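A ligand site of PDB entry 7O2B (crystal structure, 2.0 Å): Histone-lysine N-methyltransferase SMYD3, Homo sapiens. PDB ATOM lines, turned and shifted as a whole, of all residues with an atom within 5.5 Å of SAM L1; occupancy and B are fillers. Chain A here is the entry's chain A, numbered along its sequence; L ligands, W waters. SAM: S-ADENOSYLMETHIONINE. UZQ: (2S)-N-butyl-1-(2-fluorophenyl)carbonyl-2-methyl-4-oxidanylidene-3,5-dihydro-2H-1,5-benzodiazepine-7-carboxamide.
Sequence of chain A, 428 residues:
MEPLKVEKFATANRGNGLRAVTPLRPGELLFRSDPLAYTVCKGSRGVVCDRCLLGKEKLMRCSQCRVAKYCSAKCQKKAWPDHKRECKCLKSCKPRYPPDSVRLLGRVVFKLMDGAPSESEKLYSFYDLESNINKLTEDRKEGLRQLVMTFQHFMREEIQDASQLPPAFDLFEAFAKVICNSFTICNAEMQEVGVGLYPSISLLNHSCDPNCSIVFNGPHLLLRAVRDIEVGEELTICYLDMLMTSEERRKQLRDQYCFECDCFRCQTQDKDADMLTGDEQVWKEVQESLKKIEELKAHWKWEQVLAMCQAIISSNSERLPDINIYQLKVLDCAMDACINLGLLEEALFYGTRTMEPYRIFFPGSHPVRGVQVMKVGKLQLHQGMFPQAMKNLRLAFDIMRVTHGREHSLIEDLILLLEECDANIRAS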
ATOM      1  N   ASN A  13      20.874  25.943  22.700  1.00  0.00           N
ATOM      2  CA  ASN A  13      21.269  25.163  21.532  1.00  0.00           C
ATOM      3  C   ASN A  13      20.847  23.710  21.520  1.00  0.00           C
ATOM      4  O   ASN A  13      21.410  22.912  20.755  1.00  0.00           O
ATOM      5  CB  ASN A  13      22.812  25.279  21.308  1.00  0.00           C
ATOM      6  CG  ASN A  13      23.630  24.777  22.481  1.00  0.00           C
ATOM      7  OD1 ASN A  13      23.128  24.058  23.333  1.00  0.00           O
ATOM      8  ND2 ASN A  13      24.865  25.183  22.543  1.00  0.00           N
ATOM      9  N   ARG A  14      19.899  23.306  22.374  1.00  0.00           N
ATOM     10  CA  ARG A  14      19.468  21.930  22.292  1.00  0.00           C
ATOM     11  C   ARG A  14      17.944  21.778  22.463  1.00  0.00           C
ATOM     12  O   ARG A  14      17.466  20.896  23.158  1.00  0.00           O
ATOM     13  CB  ARG A  14      20.335  21.035  23.165  1.00  0.00           C
ATOM     14  CG  ARG A  14      20.143  21.133  24.624  1.00  0.00           C
ATOM     15  CD  ARG A  14      21.235  21.873  25.329  1.00  0.00           C
ATOM     16  NE  ARG A  14      22.496  21.174  25.405  1.00  0.00           N
ATOM     17  CZ  ARG A  14      22.961  20.520  26.464  1.00  0.00           C
ATOM     18  NH1 ARG A  14      24.161  19.976  26.401  1.00  0.00           N
ATOM     19  NH2 ARG A  14      22.257  20.389  27.588  1.00  0.00           N
ATOM     20  N   GLY A  15      17.226  22.631  21.738  1.00  0.00           N
ATOM     21  CA  GLY A  15      15.791  22.704  21.745  1.00  0.00           C
ATOM     22  C   GLY A  15      15.289  22.924  23.140  1.00  0.00           C
ATOM     23  O   GLY A  15      15.900  23.690  23.917  1.00  0.00           O
ATOM     24  N   ASN A  16      14.211  22.251  23.485  1.00  0.00           N
ATOM     25  CA  ASN A  16      13.601  22.370  24.799  1.00  0.00           C
ATOM     26  C   ASN A  16      14.294  21.447  25.755  1.00  0.00           C
ATOM     27  O   ASN A  16      14.849  20.468  25.316  1.00  0.00           O
ATOM     28  CB  ASN A  16      12.108  22.046  24.719  1.00  0.00           C
ATOM     29  CG  ASN A  16      11.347  23.033  23.860  1.00  0.00           C
ATOM     30  OD1 ASN A  16      10.545  22.668  22.965  1.00  0.00           O
ATOM     31  ND2 ASN A  16      11.665  24.247  24.031  1.00  0.00           N
ATOM     32  N   GLY A  17      14.161  21.723  27.065  1.00  0.00           N
ATOM     33  CA  GLY A  17      14.878  21.045  28.131  1.00  0.00           C
ATOM     34  C   GLY A  17      14.041  21.125  29.403  1.00  0.00           C
ATOM     35  O   GLY A  17      12.933  21.742  29.388  1.00  0.00           O
ATOM     36  N   TYR A 124       4.599  18.099  28.284  1.00  0.00           N
ATOM     37  CA  TYR A 124       5.006  17.999  26.895  1.00  0.00           C
ATOM     38  C   TYR A 124       4.196  16.851  26.350  1.00  0.00           C
ATOM     39  O   TYR A 124       4.042  15.827  27.017  1.00  0.00           O
ATOM     40  CB  TYR A 124       6.490  17.640  26.792  1.00  0.00           C
ATOM     41  CG  TYR A 124       7.346  18.177  25.635  1.00  0.00           C
ATOM     42  CD1 TYR A 124       7.230  19.494  25.147  1.00  0.00           C
ATOM     43  CD2 TYR A 124       8.338  17.382  25.097  1.00  0.00           C
ATOM     44  CE1 TYR A 124       8.080  19.964  24.181  1.00  0.00           C
ATOM     45  CE2 TYR A 124       9.175  17.844  24.106  1.00  0.00           C
ATOM     46  CZ  TYR A 124       9.076  19.125  23.676  1.00  0.00           C
ATOM     47  OH  TYR A 124       9.964  19.499  22.687  1.00  0.00           O
ATOM     48  N   ASP A 128       4.196  17.728  20.617  1.00  0.00           N
ATOM     49  CA  ASP A 128       5.358  18.609  20.793  1.00  0.00           C
ATOM     50  C   ASP A 128       6.724  17.910  20.583  1.00  0.00           C
ATOM     51  O   ASP A 128       7.750  18.560  20.556  1.00  0.00           O
ATOM     52  CB  ASP A 128       5.403  19.157  22.221  1.00  0.00           C
ATOM     53  CG  ASP A 128       4.153  19.928  22.625  1.00  0.00           C
ATOM     54  OD1 ASP A 128       3.675  20.722  21.816  1.00  0.00           O
ATOM     55  OD2 ASP A 128       3.711  19.753  23.790  1.00  0.00           O
ATOM     56  N   LEU A 129       6.769  16.591  20.579  1.00  0.00           N
ATOM     57  CA  LEU A 129       8.064  15.910  20.621  1.00  0.00           C
ATOM     58  C   LEU A 129       9.001  16.326  19.461  1.00  0.00           C
ATOM     59  O   LEU A 129       8.575  16.649  18.341  1.00  0.00           O
ATOM     60  CB  LEU A 129       7.889  14.402  20.587  1.00  0.00           C
ATOM     61  CG  LEU A 129       7.279  13.721  21.812  1.00  0.00           C
ATOM     62  CD1 LEU A 129       7.256  12.227  21.572  1.00  0.00           C
ATOM     63  CD2 LEU A 129       8.044  14.062  23.080  1.00  0.00           C
ATOM     64  N   GLU A 130      10.291  16.259  19.721  1.00  0.00           N
ATOM     65  CA  GLU A 130      11.276  16.559  18.718  1.00  0.00           C
ATOM     66  C   GLU A 130      11.309  15.473  17.622  1.00  0.00           C
ATOM     67  O   GLU A 130      11.323  14.270  17.908  1.00  0.00           O
ATOM     68  CB  GLU A 130      12.663  16.663  19.422  1.00  0.00           C
ATOM     69  CG  GLU A 130      13.832  16.883  18.461  1.00  0.00           C
ATOM     70  CD  GLU A 130      13.754  18.209  17.747  1.00  0.00           C
ATOM     71  OE1 GLU A 130      14.001  19.236  18.455  1.00  0.00           O
ATOM     72  OE2 GLU A 130      13.478  18.227  16.524  1.00  0.00           O
ATOM     73  N   ASN A 132      13.631  16.053  14.732  1.00  0.00           N
ATOM     74  CA  ASN A 132      14.891  16.275  13.989  1.00  0.00           C
ATOM     75  C   ASN A 132      14.700  16.124  12.500  1.00  0.00           C
ATOM     76  O   ASN A 132      15.587  15.621  11.837  1.00  0.00           O
ATOM     77  CB  ASN A 132      16.003  15.321  14.449  1.00  0.00           C
ATOM     78  CG  ASN A 132      16.328  15.487  15.895  1.00  0.00           C
ATOM     79  OD1 ASN A 132      16.712  16.540  16.311  1.00  0.00           O
ATOM     80  ND2 ASN A 132      16.099  14.464  16.694  1.00  0.00           N
ATOM     81  N   CYS A 180      13.825   9.139  18.286  1.00  0.00           N
ATOM     82  CA  CYS A 180      14.600   9.881  19.244  1.00  0.00           C
ATOM     83  C   CYS A 180      13.869  10.182  20.562  1.00  0.00           C
ATOM     84  O   CYS A 180      14.340  11.004  21.319  1.00  0.00           O
ATOM     85  CB  CYS A 180      15.110  11.152  18.615  1.00  0.00           C
ATOM     86  SG  CYS A 180      13.879  12.421  18.267  1.00  0.00           S
ATOM     87  N   ASN A 181      12.736   9.540  20.809  1.00  0.00           N
ATOM     88  CA  ASN A 181      12.011   9.671  22.104  1.00  0.00           C
ATOM     89  C   ASN A 181      11.571   8.337  22.733  1.00  0.00           C
ATOM     90  O   ASN A 181      10.746   8.330  23.642  1.00  0.00           O
ATOM     91  CB  ASN A 181      10.803  10.592  21.957  1.00  0.00           C
ATOM     92  CG  ASN A 181      11.202  12.010  21.660  1.00  0.00           C
ATOM     93  OD1 ASN A 181      11.569  12.757  22.595  1.00  0.00           O
ATOM     94  ND2 ASN A 181      11.157  12.411  20.391  1.00  0.00           N
ATOM     95  N   SER A 202      10.491  13.241  28.066  1.00  0.00           N
ATOM     96  CA  SER A 202      11.223  13.369  26.847  1.00  0.00           C
ATOM     97  C   SER A 202      11.895  14.750  26.727  1.00  0.00           C
ATOM     98  O   SER A 202      12.733  14.929  25.861  1.00  0.00           O
ATOM     99  CB  SER A 202      10.270  13.219  25.645  1.00  0.00           C
ATOM    100  OG  SER A 202      10.169  11.903  25.259  1.00  0.00           O
ATOM    101  N   LEU A 203      11.495  15.715  27.550  1.00  0.00           N
ATOM    102  CA  LEU A 203      12.213  16.983  27.638  1.00  0.00           C
ATOM    103  C   LEU A 203      13.649  16.834  28.082  1.00  0.00           C
ATOM    104  O   LEU A 203      14.427  17.716  27.800  1.00  0.00           O
ATOM    105  CB  LEU A 203      11.489  17.962  28.602  1.00  0.00           C
ATOM    106  CG  LEU A 203      10.187  18.556  28.008  1.00  0.00           C
ATOM    107  CD1 LEU A 203       9.291  19.145  29.131  1.00  0.00           C
ATOM    108  CD2 LEU A 203      10.523  19.588  26.988  1.00  0.00           C
ATOM    109  N   LEU A 204      14.012  15.758  28.784  1.00  0.00           N
ATOM    110  CA  LEU A 204      15.390  15.624  29.292  1.00  0.00           C
ATOM    111  C   LEU A 204      16.358  15.510  28.155  1.00  0.00           C
ATOM    112  O   LEU A 204      16.254  14.554  27.340  1.00  0.00           O
ATOM    113  CB  LEU A 204      15.565  14.380  30.186  1.00  0.00           C
ATOM    114  CG  LEU A 204      14.735  14.474  31.489  1.00  0.00           C
ATOM    115  CD1 LEU A 204      14.592  13.076  32.088  1.00  0.00           C
ATOM    116  CD2 LEU A 204      15.383  15.393  32.486  1.00  0.00           C
ATOM    117  N   ASN A 205      17.306  16.454  28.105  1.00  0.00           N
ATOM    118  CA  ASN A 205      18.442  16.297  27.195  1.00  0.00           C
ATOM    119  C   ASN A 205      19.486  15.362  27.797  1.00  0.00           C
ATOM    120  O   ASN A 205      19.480  15.081  29.010  1.00  0.00           O
ATOM    121  CB  ASN A 205      19.035  17.633  26.803  1.00  0.00           C
ATOM    122  CG  ASN A 205      18.107  18.411  25.885  1.00  0.00           C
ATOM    123  OD1 ASN A 205      17.627  17.901  24.889  1.00  0.00           O
ATOM    124  ND2 ASN A 205      17.872  19.661  26.219  1.00  0.00           N
ATOM    125  N   HIS A 206      20.344  14.885  26.902  1.00  0.00           N
ATOM    126  CA  HIS A 206      21.459  13.958  27.208  1.00  0.00           C
ATOM    127  C   HIS A 206      22.692  14.596  27.830  1.00  0.00           C
ATOM    128  O   HIS A 206      23.139  15.646  27.410  1.00  0.00           O
ATOM    129  CB  HIS A 206      21.919  13.294  25.922  1.00  0.00           C
ATOM    130  CG  HIS A 206      23.217  12.554  26.048  1.00  0.00           C
ATOM    131  ND1 HIS A 206      23.321  11.335  26.662  1.00  0.00           N
ATOM    132  CD2 HIS A 206      24.471  12.874  25.661  1.00  0.00           C
ATOM    133  CE1 HIS A 206      24.565  10.901  26.631  1.00  0.00           C
ATOM    134  NE2 HIS A 206      25.298  11.822  26.033  1.00  0.00           N
ATOM    135  N   SER A 207      23.334  13.897  28.736  1.00  0.00           N
ATOM    136  CA  SER A 207      24.669  14.259  29.130  1.00  0.00           C
ATOM    137  C   SER A 207      25.449  12.980  29.362  1.00  0.00           C
ATOM    138  O   SER A 207      24.897  11.990  29.875  1.00  0.00           O
ATOM    139  CB  SER A 207      24.642  15.083  30.412  1.00  0.00           C
ATOM    140  OG  SER A 207      25.930  15.100  30.957  1.00  0.00           O
ATOM    141  N   TYR A 239      21.500   9.027  27.938  1.00  0.00           N
ATOM    142  CA  TYR A 239      20.631   8.257  27.064  1.00  0.00           C
ATOM    143  C   TYR A 239      21.229   6.866  26.766  1.00  0.00           C
ATOM    144  O   TYR A 239      20.510   5.949  26.279  1.00  0.00           O
ATOM    145  CB  TYR A 239      20.470   8.963  25.717  1.00  0.00           C
ATOM    146  CG  TYR A 239      19.689  10.260  25.632  1.00  0.00           C
ATOM    147  CD1 TYR A 239      19.084  10.827  26.715  1.00  0.00           C
ATOM    148  CD2 TYR A 239      19.518  10.884  24.394  1.00  0.00           C
ATOM    149  CE1 TYR A 239      18.353  12.017  26.596  1.00  0.00           C
ATOM    150  CE2 TYR A 239      18.804  12.063  24.251  1.00  0.00           C
ATOM    151  CZ  TYR A 239      18.214  12.632  25.368  1.00  0.00           C
ATOM    152  OH  TYR A 239      17.445  13.765  25.225  1.00  0.00           O
ATOM    153  N   GLN A 256      20.840   8.103  15.930  1.00  0.00           N
ATOM    154  CA  GLN A 256      19.548   8.042  16.564  1.00  0.00           C
ATOM    155  C   GLN A 256      19.023   9.417  17.001  1.00  0.00           C
ATOM    156  O   GLN A 256      17.818   9.640  16.924  1.00  0.00           O
ATOM    157  CB  GLN A 256      19.643   7.097  17.781  1.00  0.00           C
ATOM    158  CG  GLN A 256      18.329   6.864  18.509  1.00  0.00           C
ATOM    159  CD  GLN A 256      18.319   5.661  19.496  1.00  0.00           C
ATOM    160  OE1 GLN A 256      19.357   5.088  19.828  1.00  0.00           O
ATOM    161  NE2 GLN A 256      17.139   5.310  19.964  1.00  0.00           N
ATOM    162  N   TYR A 257      19.888  10.301  17.510  1.00  0.00           N
ATOM    163  CA  TYR A 257      19.474  11.567  18.101  1.00  0.00           C
ATOM    164  C   TYR A 257      19.876  12.832  17.330  1.00  0.00           C
ATOM    165  O   TYR A 257      19.464  13.952  17.682  1.00  0.00           O
ATOM    166  CB  TYR A 257      19.983  11.655  19.529  1.00  0.00           C
ATOM    167  CG  TYR A 257      19.407  10.558  20.384  1.00  0.00           C
ATOM    168  CD1 TYR A 257      18.106  10.650  20.850  1.00  0.00           C
ATOM    169  CD2 TYR A 257      20.149   9.396  20.675  1.00  0.00           C
ATOM    170  CE1 TYR A 257      17.566   9.662  21.617  1.00  0.00           C
ATOM    171  CE2 TYR A 257      19.611   8.390  21.444  1.00  0.00           C
ATOM    172  CZ  TYR A 257      18.288   8.526  21.894  1.00  0.00           C
ATOM    173  OH  TYR A 257      17.677   7.567  22.677  1.00  0.00           O
ATOM    174  N   CYS A 258      20.641  12.647  16.269  1.00  0.00           N
ATOM    175  CA  CYS A 258      21.030  13.744  15.395  1.00  0.00           C
ATOM    176  C   CYS A 258      21.670  14.865  16.157  1.00  0.00           C
ATOM    177  O   CYS A 258      21.335  16.031  15.918  1.00  0.00           O
ATOM    178  CB  CYS A 258      19.800  14.297  14.669  1.00  0.00           C
ATOM    179  SG  CYS A 258      19.167  13.208  13.415  1.00  0.00           S
ATOM    180  N   PHE A 259      22.567  14.561  17.089  1.00  0.00           N
ATOM    181  CA  PHE A 259      23.435  15.638  17.609  1.00  0.00           C
ATOM    182  C   PHE A 259      24.851  15.201  17.915  1.00  0.00           C
ATOM    183  O   PHE A 259      25.122  13.992  17.975  1.00  0.00           O
ATOM    184  CB  PHE A 259      22.834  16.310  18.831  1.00  0.00           C
ATOM    185  CG  PHE A 259      22.932  15.506  20.074  1.00  0.00           C
ATOM    186  CD1 PHE A 259      24.031  15.664  20.958  1.00  0.00           C
ATOM    187  CD2 PHE A 259      21.946  14.573  20.386  1.00  0.00           C
ATOM    188  CE1 PHE A 259      24.077  14.898  22.118  1.00  0.00           C
ATOM    189  CE2 PHE A 259      22.022  13.837  21.532  1.00  0.00           C
ATOM    190  CZ  PHE A 259      23.075  13.990  22.402  1.00  0.00           C
ATOM    191  N   GLU A 260      25.730  16.205  18.020  1.00  0.00           N
ATOM    192  CA  GLU A 260      27.147  16.062  18.267  1.00  0.00           C
ATOM    193  C   GLU A 260      27.413  16.502  19.733  1.00  0.00           C
ATOM    194  O   GLU A 260      26.905  17.537  20.170  1.00  0.00           O
ATOM    195  CB  GLU A 260      27.918  16.989  17.297  1.00  0.00           C
ATOM    196  CG  GLU A 260      27.368  16.920  15.856  1.00  0.00           C
ATOM    197  CD  GLU A 260      27.712  15.636  15.128  1.00  0.00           C
ATOM    198  OE1 GLU A 260      28.540  14.812  15.656  1.00  0.00           O
ATOM    199  OE2 GLU A 260      27.183  15.463  14.006  1.00  0.00           O
ATOM    200  N   CYS A 261      28.110  15.703  20.510  1.00  0.00           N
ATOM    201  CA  CYS A 261      28.381  16.066  21.913  1.00  0.00           C
ATOM    202  C   CYS A 261      29.783  16.610  22.013  1.00  0.00           C
ATOM    203  O   CYS A 261      30.720  15.942  21.560  1.00  0.00           O
ATOM    204  CB  CYS A 261      28.234  14.865  22.845  1.00  0.00           C
ATOM    205  SG  CYS A 261      28.302  15.344  24.613  1.00  0.00           S
HETATM  206  N   SAM L   1      15.602  18.706  23.180  1.00  0.00           N
HETATM  207  CA  SAM L   1      14.433  17.852  22.987  1.00  0.00           C
HETATM  208  C   SAM L   1      13.177  18.623  22.600  1.00  0.00           C
HETATM  209  O   SAM L   1      13.311  19.782  22.219  1.00  0.00           O
HETATM  210  OXT SAM L   1      12.053  18.076  22.648  1.00  0.00           O
HETATM  211  CB  SAM L   1      14.188  17.026  24.256  1.00  0.00           C
HETATM  212  CG  SAM L   1      15.109  15.785  24.299  1.00  0.00           C
HETATM  213  SD  SAM L   1      14.640  14.615  23.213  1.00  0.00           S
HETATM  214  CE  SAM L   1      14.296  13.288  24.172  1.00  0.00           C
HETATM  215  C5' SAM L   1      15.995  14.161  22.272  1.00  0.00           C
HETATM  216  C4' SAM L   1      16.581  15.233  21.361  1.00  0.00           C
HETATM  217  O4' SAM L   1      17.035  16.347  22.075  1.00  0.00           O
HETATM  218  C3' SAM L   1      17.794  14.828  20.480  1.00  0.00           C
HETATM  219  O3' SAM L   1      17.467  14.010  19.330  1.00  0.00           O
HETATM  220  C2' SAM L   1      18.424  16.131  20.165  1.00  0.00           C
HETATM  221  O2' SAM L   1      17.649  16.886  19.212  1.00  0.00           O
HETATM  222  C1' SAM L   1      18.214  16.859  21.478  1.00  0.00           C
HETATM  223  N9  SAM L   1      19.343  16.699  22.444  1.00  0.00           N
HETATM  224  C8  SAM L   1      19.316  15.953  23.554  1.00  0.00           C
HETATM  225  N7  SAM L   1      20.456  16.063  24.237  1.00  0.00           N
HETATM  226  C5  SAM L   1      21.239  16.908  23.552  1.00  0.00           C
HETATM  227  C6  SAM L   1      22.571  17.484  23.704  1.00  0.00           C
HETATM  228  N6  SAM L   1      23.332  17.123  24.775  1.00  0.00           N
HETATM  229  N1  SAM L   1      23.017  18.378  22.735  1.00  0.00           N
HETATM  230  C2  SAM L   1      22.252  18.746  21.707  1.00  0.00           C
HETATM  231  N3  SAM L   1      21.018  18.246  21.500  1.00  0.00           N
HETATM  232  C4  SAM L   1      20.488  17.339  22.364  1.00  0.00           C
HETATM  233  C4  UZQ L   2      16.592   3.636  29.522  1.00  0.00           C
HETATM  234  C5  UZQ L   2      17.364   4.521  28.744  1.00  0.00           C
HETATM  235  C6  UZQ L   2      18.752   4.493  28.914  1.00  0.00           C
HETATM  236  C7  UZQ L   2      16.665   5.383  27.714  1.00  0.00           C
HETATM  237  C10 UZQ L   2      16.926   7.056  25.853  1.00  0.00           C
HETATM  238  C13 UZQ L   2      14.655   9.192  24.811  1.00  0.00           C
HETATM  239  C15 UZQ L   2      16.512   1.724  32.422  1.00  0.00           C
HETATM  240  C17 UZQ L   2      18.960   1.919  32.895  1.00  0.00           C
HETATM  241  C20 UZQ L   2      19.971   2.890  33.489  1.00  0.00           C
HETATM  242  C21 UZQ L   2      19.951   0.884  30.964  1.00  0.00           C
HETATM  243  C24 UZQ L   2      21.480   1.078  29.003  1.00  0.00           C
HETATM  244  C26 UZQ L   2      20.704   0.649  26.695  1.00  0.00           C
HETATM  245  C28 UZQ L   2      19.221   0.453  28.545  1.00  0.00           C
HETATM  246  C12 UZQ L   2      16.014   9.362  25.394  1.00  0.00           C
HETATM  247  C11 UZQ L   2      16.302   8.298  26.442  1.00  0.00           C
HETATM  248  N9  UZQ L   2      17.429   6.210  26.950  1.00  0.00           N
HETATM  249  O8  UZQ L   2      15.539   5.038  27.403  1.00  0.00           O
HETATM  250  C1  UZQ L   2      19.369   3.602  29.839  1.00  0.00           C
HETATM  251  C2  UZQ L   2      18.593   2.727  30.601  1.00  0.00           C
HETATM  252  C3  UZQ L   2      17.214   2.756  30.441  1.00  0.00           C
HETATM  253  N14 UZQ L   2      16.394   1.937  31.130  1.00  0.00           N
HETATM  254  O19 UZQ L   2      15.743   0.900  32.934  1.00  0.00           O
HETATM  255  C16 UZQ L   2      17.578   2.471  33.200  1.00  0.00           C
HETATM  256  N18 UZQ L   2      19.228   1.902  31.441  1.00  0.00           N
HETATM  257  O22 UZQ L   2      20.583   0.112  31.692  1.00  0.00           O
HETATM  258  C23 UZQ L   2      20.221   0.802  29.468  1.00  0.00           C
HETATM  259  C25 UZQ L   2      21.693   0.991  27.630  1.00  0.00           C
HETATM  260  C27 UZQ L   2      19.448   0.379  27.176  1.00  0.00           C
HETATM  261  F29 UZQ L   2      17.996   0.166  28.969  1.00  0.00           F
HETATM  262  O   HOH W   1      20.484  19.419  19.022  1.00  0.00           O
HETATM  263  O   HOH W   2      12.182  20.524  19.925  1.00  0.00           O
HETATM  264  O   HOH W   3      19.440  17.552  17.094  1.00  0.00           O
HETATM  265  O   HOH W   4      25.631  19.125  22.277  1.00  0.00           O
HETATM  266  O   HOH W   5      15.953  19.079  20.473  1.00  0.00           O
HETATM  267  O   HOH W   6      11.089  15.604  22.240  1.00  0.00           O
HETATM  268  O   HOH W   7      26.258  17.482  25.162  1.00  0.00           O
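ND2 of Asn 205 lies within hydrogen-bond range of O of Asn 16 (3.3 Å). The backbone NH (N) of Tyr 239 sits at hydrogen-bond distance from a ring nitrogen (ND1) of His 206 (3.2 Å). The backbone NH (N) of Asn 132 is in hydrogen-bond range of the side-chain carboxylate (OE2) of Glu 130, 2.8 Å away. The side-chain amide nitrogen of Asn 132 is in hydrogen-bond range of the side-chain sulfur of Cys 180. The backbone carbonyl oxygen (O) of Glu 130 is in hydrogen-bond range of the side-chain amide nitrogen (ND2) of Asn 181 (3.1 Å). ND2 of Asn 181 lies within hydrogen-bond range of SG of Cys 180 (3.5 Å). The side-chain hydroxyl (OH) of Tyr 239 lies within hydrogen-bond range of the backbone carbonyl oxygen (O) of Leu 204 (2.6 Å). O of Glu 130 lies within hydrogen-bond range of SG of Cys 180 (3.2 Å).
Water W2 lies within hydrogen-bond range of O of SAM L1 (2.7 Å) and OE1 of Glu 130 (2.7 Å). Water W6 lies within hydrogen-bond range of OXT of SAM L1, N of Glu 130 and OD1 of Asn 181. Water W5 bridges N of SAM L1 (2.8 Å) and OE1 of Glu 130 (2.8 Å). Water W4 bridges N1 of SAM L1 (2.8 Å) and O of Glu 260 (2.9 Å). Water W3 lies within hydrogen-bond range of O of Cys 258, O2' of SAM L1 and OD1 of Asn 132. Water W7 lies within hydrogen-bond range of N6 of SAM L1 and NH1 of Arg 14.
OXT of SAM L1 lies within hydrogen-bond range of OH of Tyr 124, 2.5 Å away. An oxygen (O3') of SAM L1 is in hydrogen-bond range of the backbone carbonyl oxygen (O) of Tyr 257. The side-chain amide oxygen (OD1) of Asn 205 sits at hydrogen-bond distance from a nitrogen (N) of SAM L1 (2.8 Å). O of SAM L1 is in hydrogen-bond range of N of Asn 16. The backbone carbonyl oxygen (O) of Asn 16 sits at hydrogen-bond distance from a nitrogen (N) of SAM L1 (2.9 Å). O of Arg 14 sits at hydrogen-bond distance from N of SAM L1. The backbone NH (N) of His 206 lies within hydrogen-bond range of a nitrogen (N7) of SAM L1 (2.9 Å). The backbone carbonyl oxygen (O) of His 206 sits at hydrogen-bond distance from a nitrogen (N6) of SAM L1. An oxygen (O3') of SAM L1 is in hydrogen-bond range of the side-chain amide nitrogen (ND2) of Asn 132 (3.0 Å). A nitrogen (N9) of UZQ L2 sits at hydrogen-bond distance from the backbone carbonyl oxygen of Tyr 239, 3.2 Å away.
A sulfur (SD) of SAM L1 lies close to the side-chain amide oxygen of Asn 181, 3.6 Å away. O of Ser 202 lies close to SD of SAM L1 (3.3 Å). OH of Tyr 239 sits close to SD of SAM L1 (3.6 Å). Gly 15 touches SAM L1 (C to O, 3.8 Å). Glu 130 touches SAM L1. Cys 180 touches SAM L1. Leu 203 touches SAM L1 (O to CB, 3.6 Å). Leu 204 touches SAM L1 (O to CG, 3.5 Å). Phe 259 touches SAM L1. Within 4 Å of SAM L1: Arg 14, Gly 15, Asn 16, Tyr 124, Glu 130, Asn 132, Cys 180, Asn 181, Ser 202, Leu 203, Leu 204, Asn 205, His 206, Tyr 239, Tyr 257 and Phe 259.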
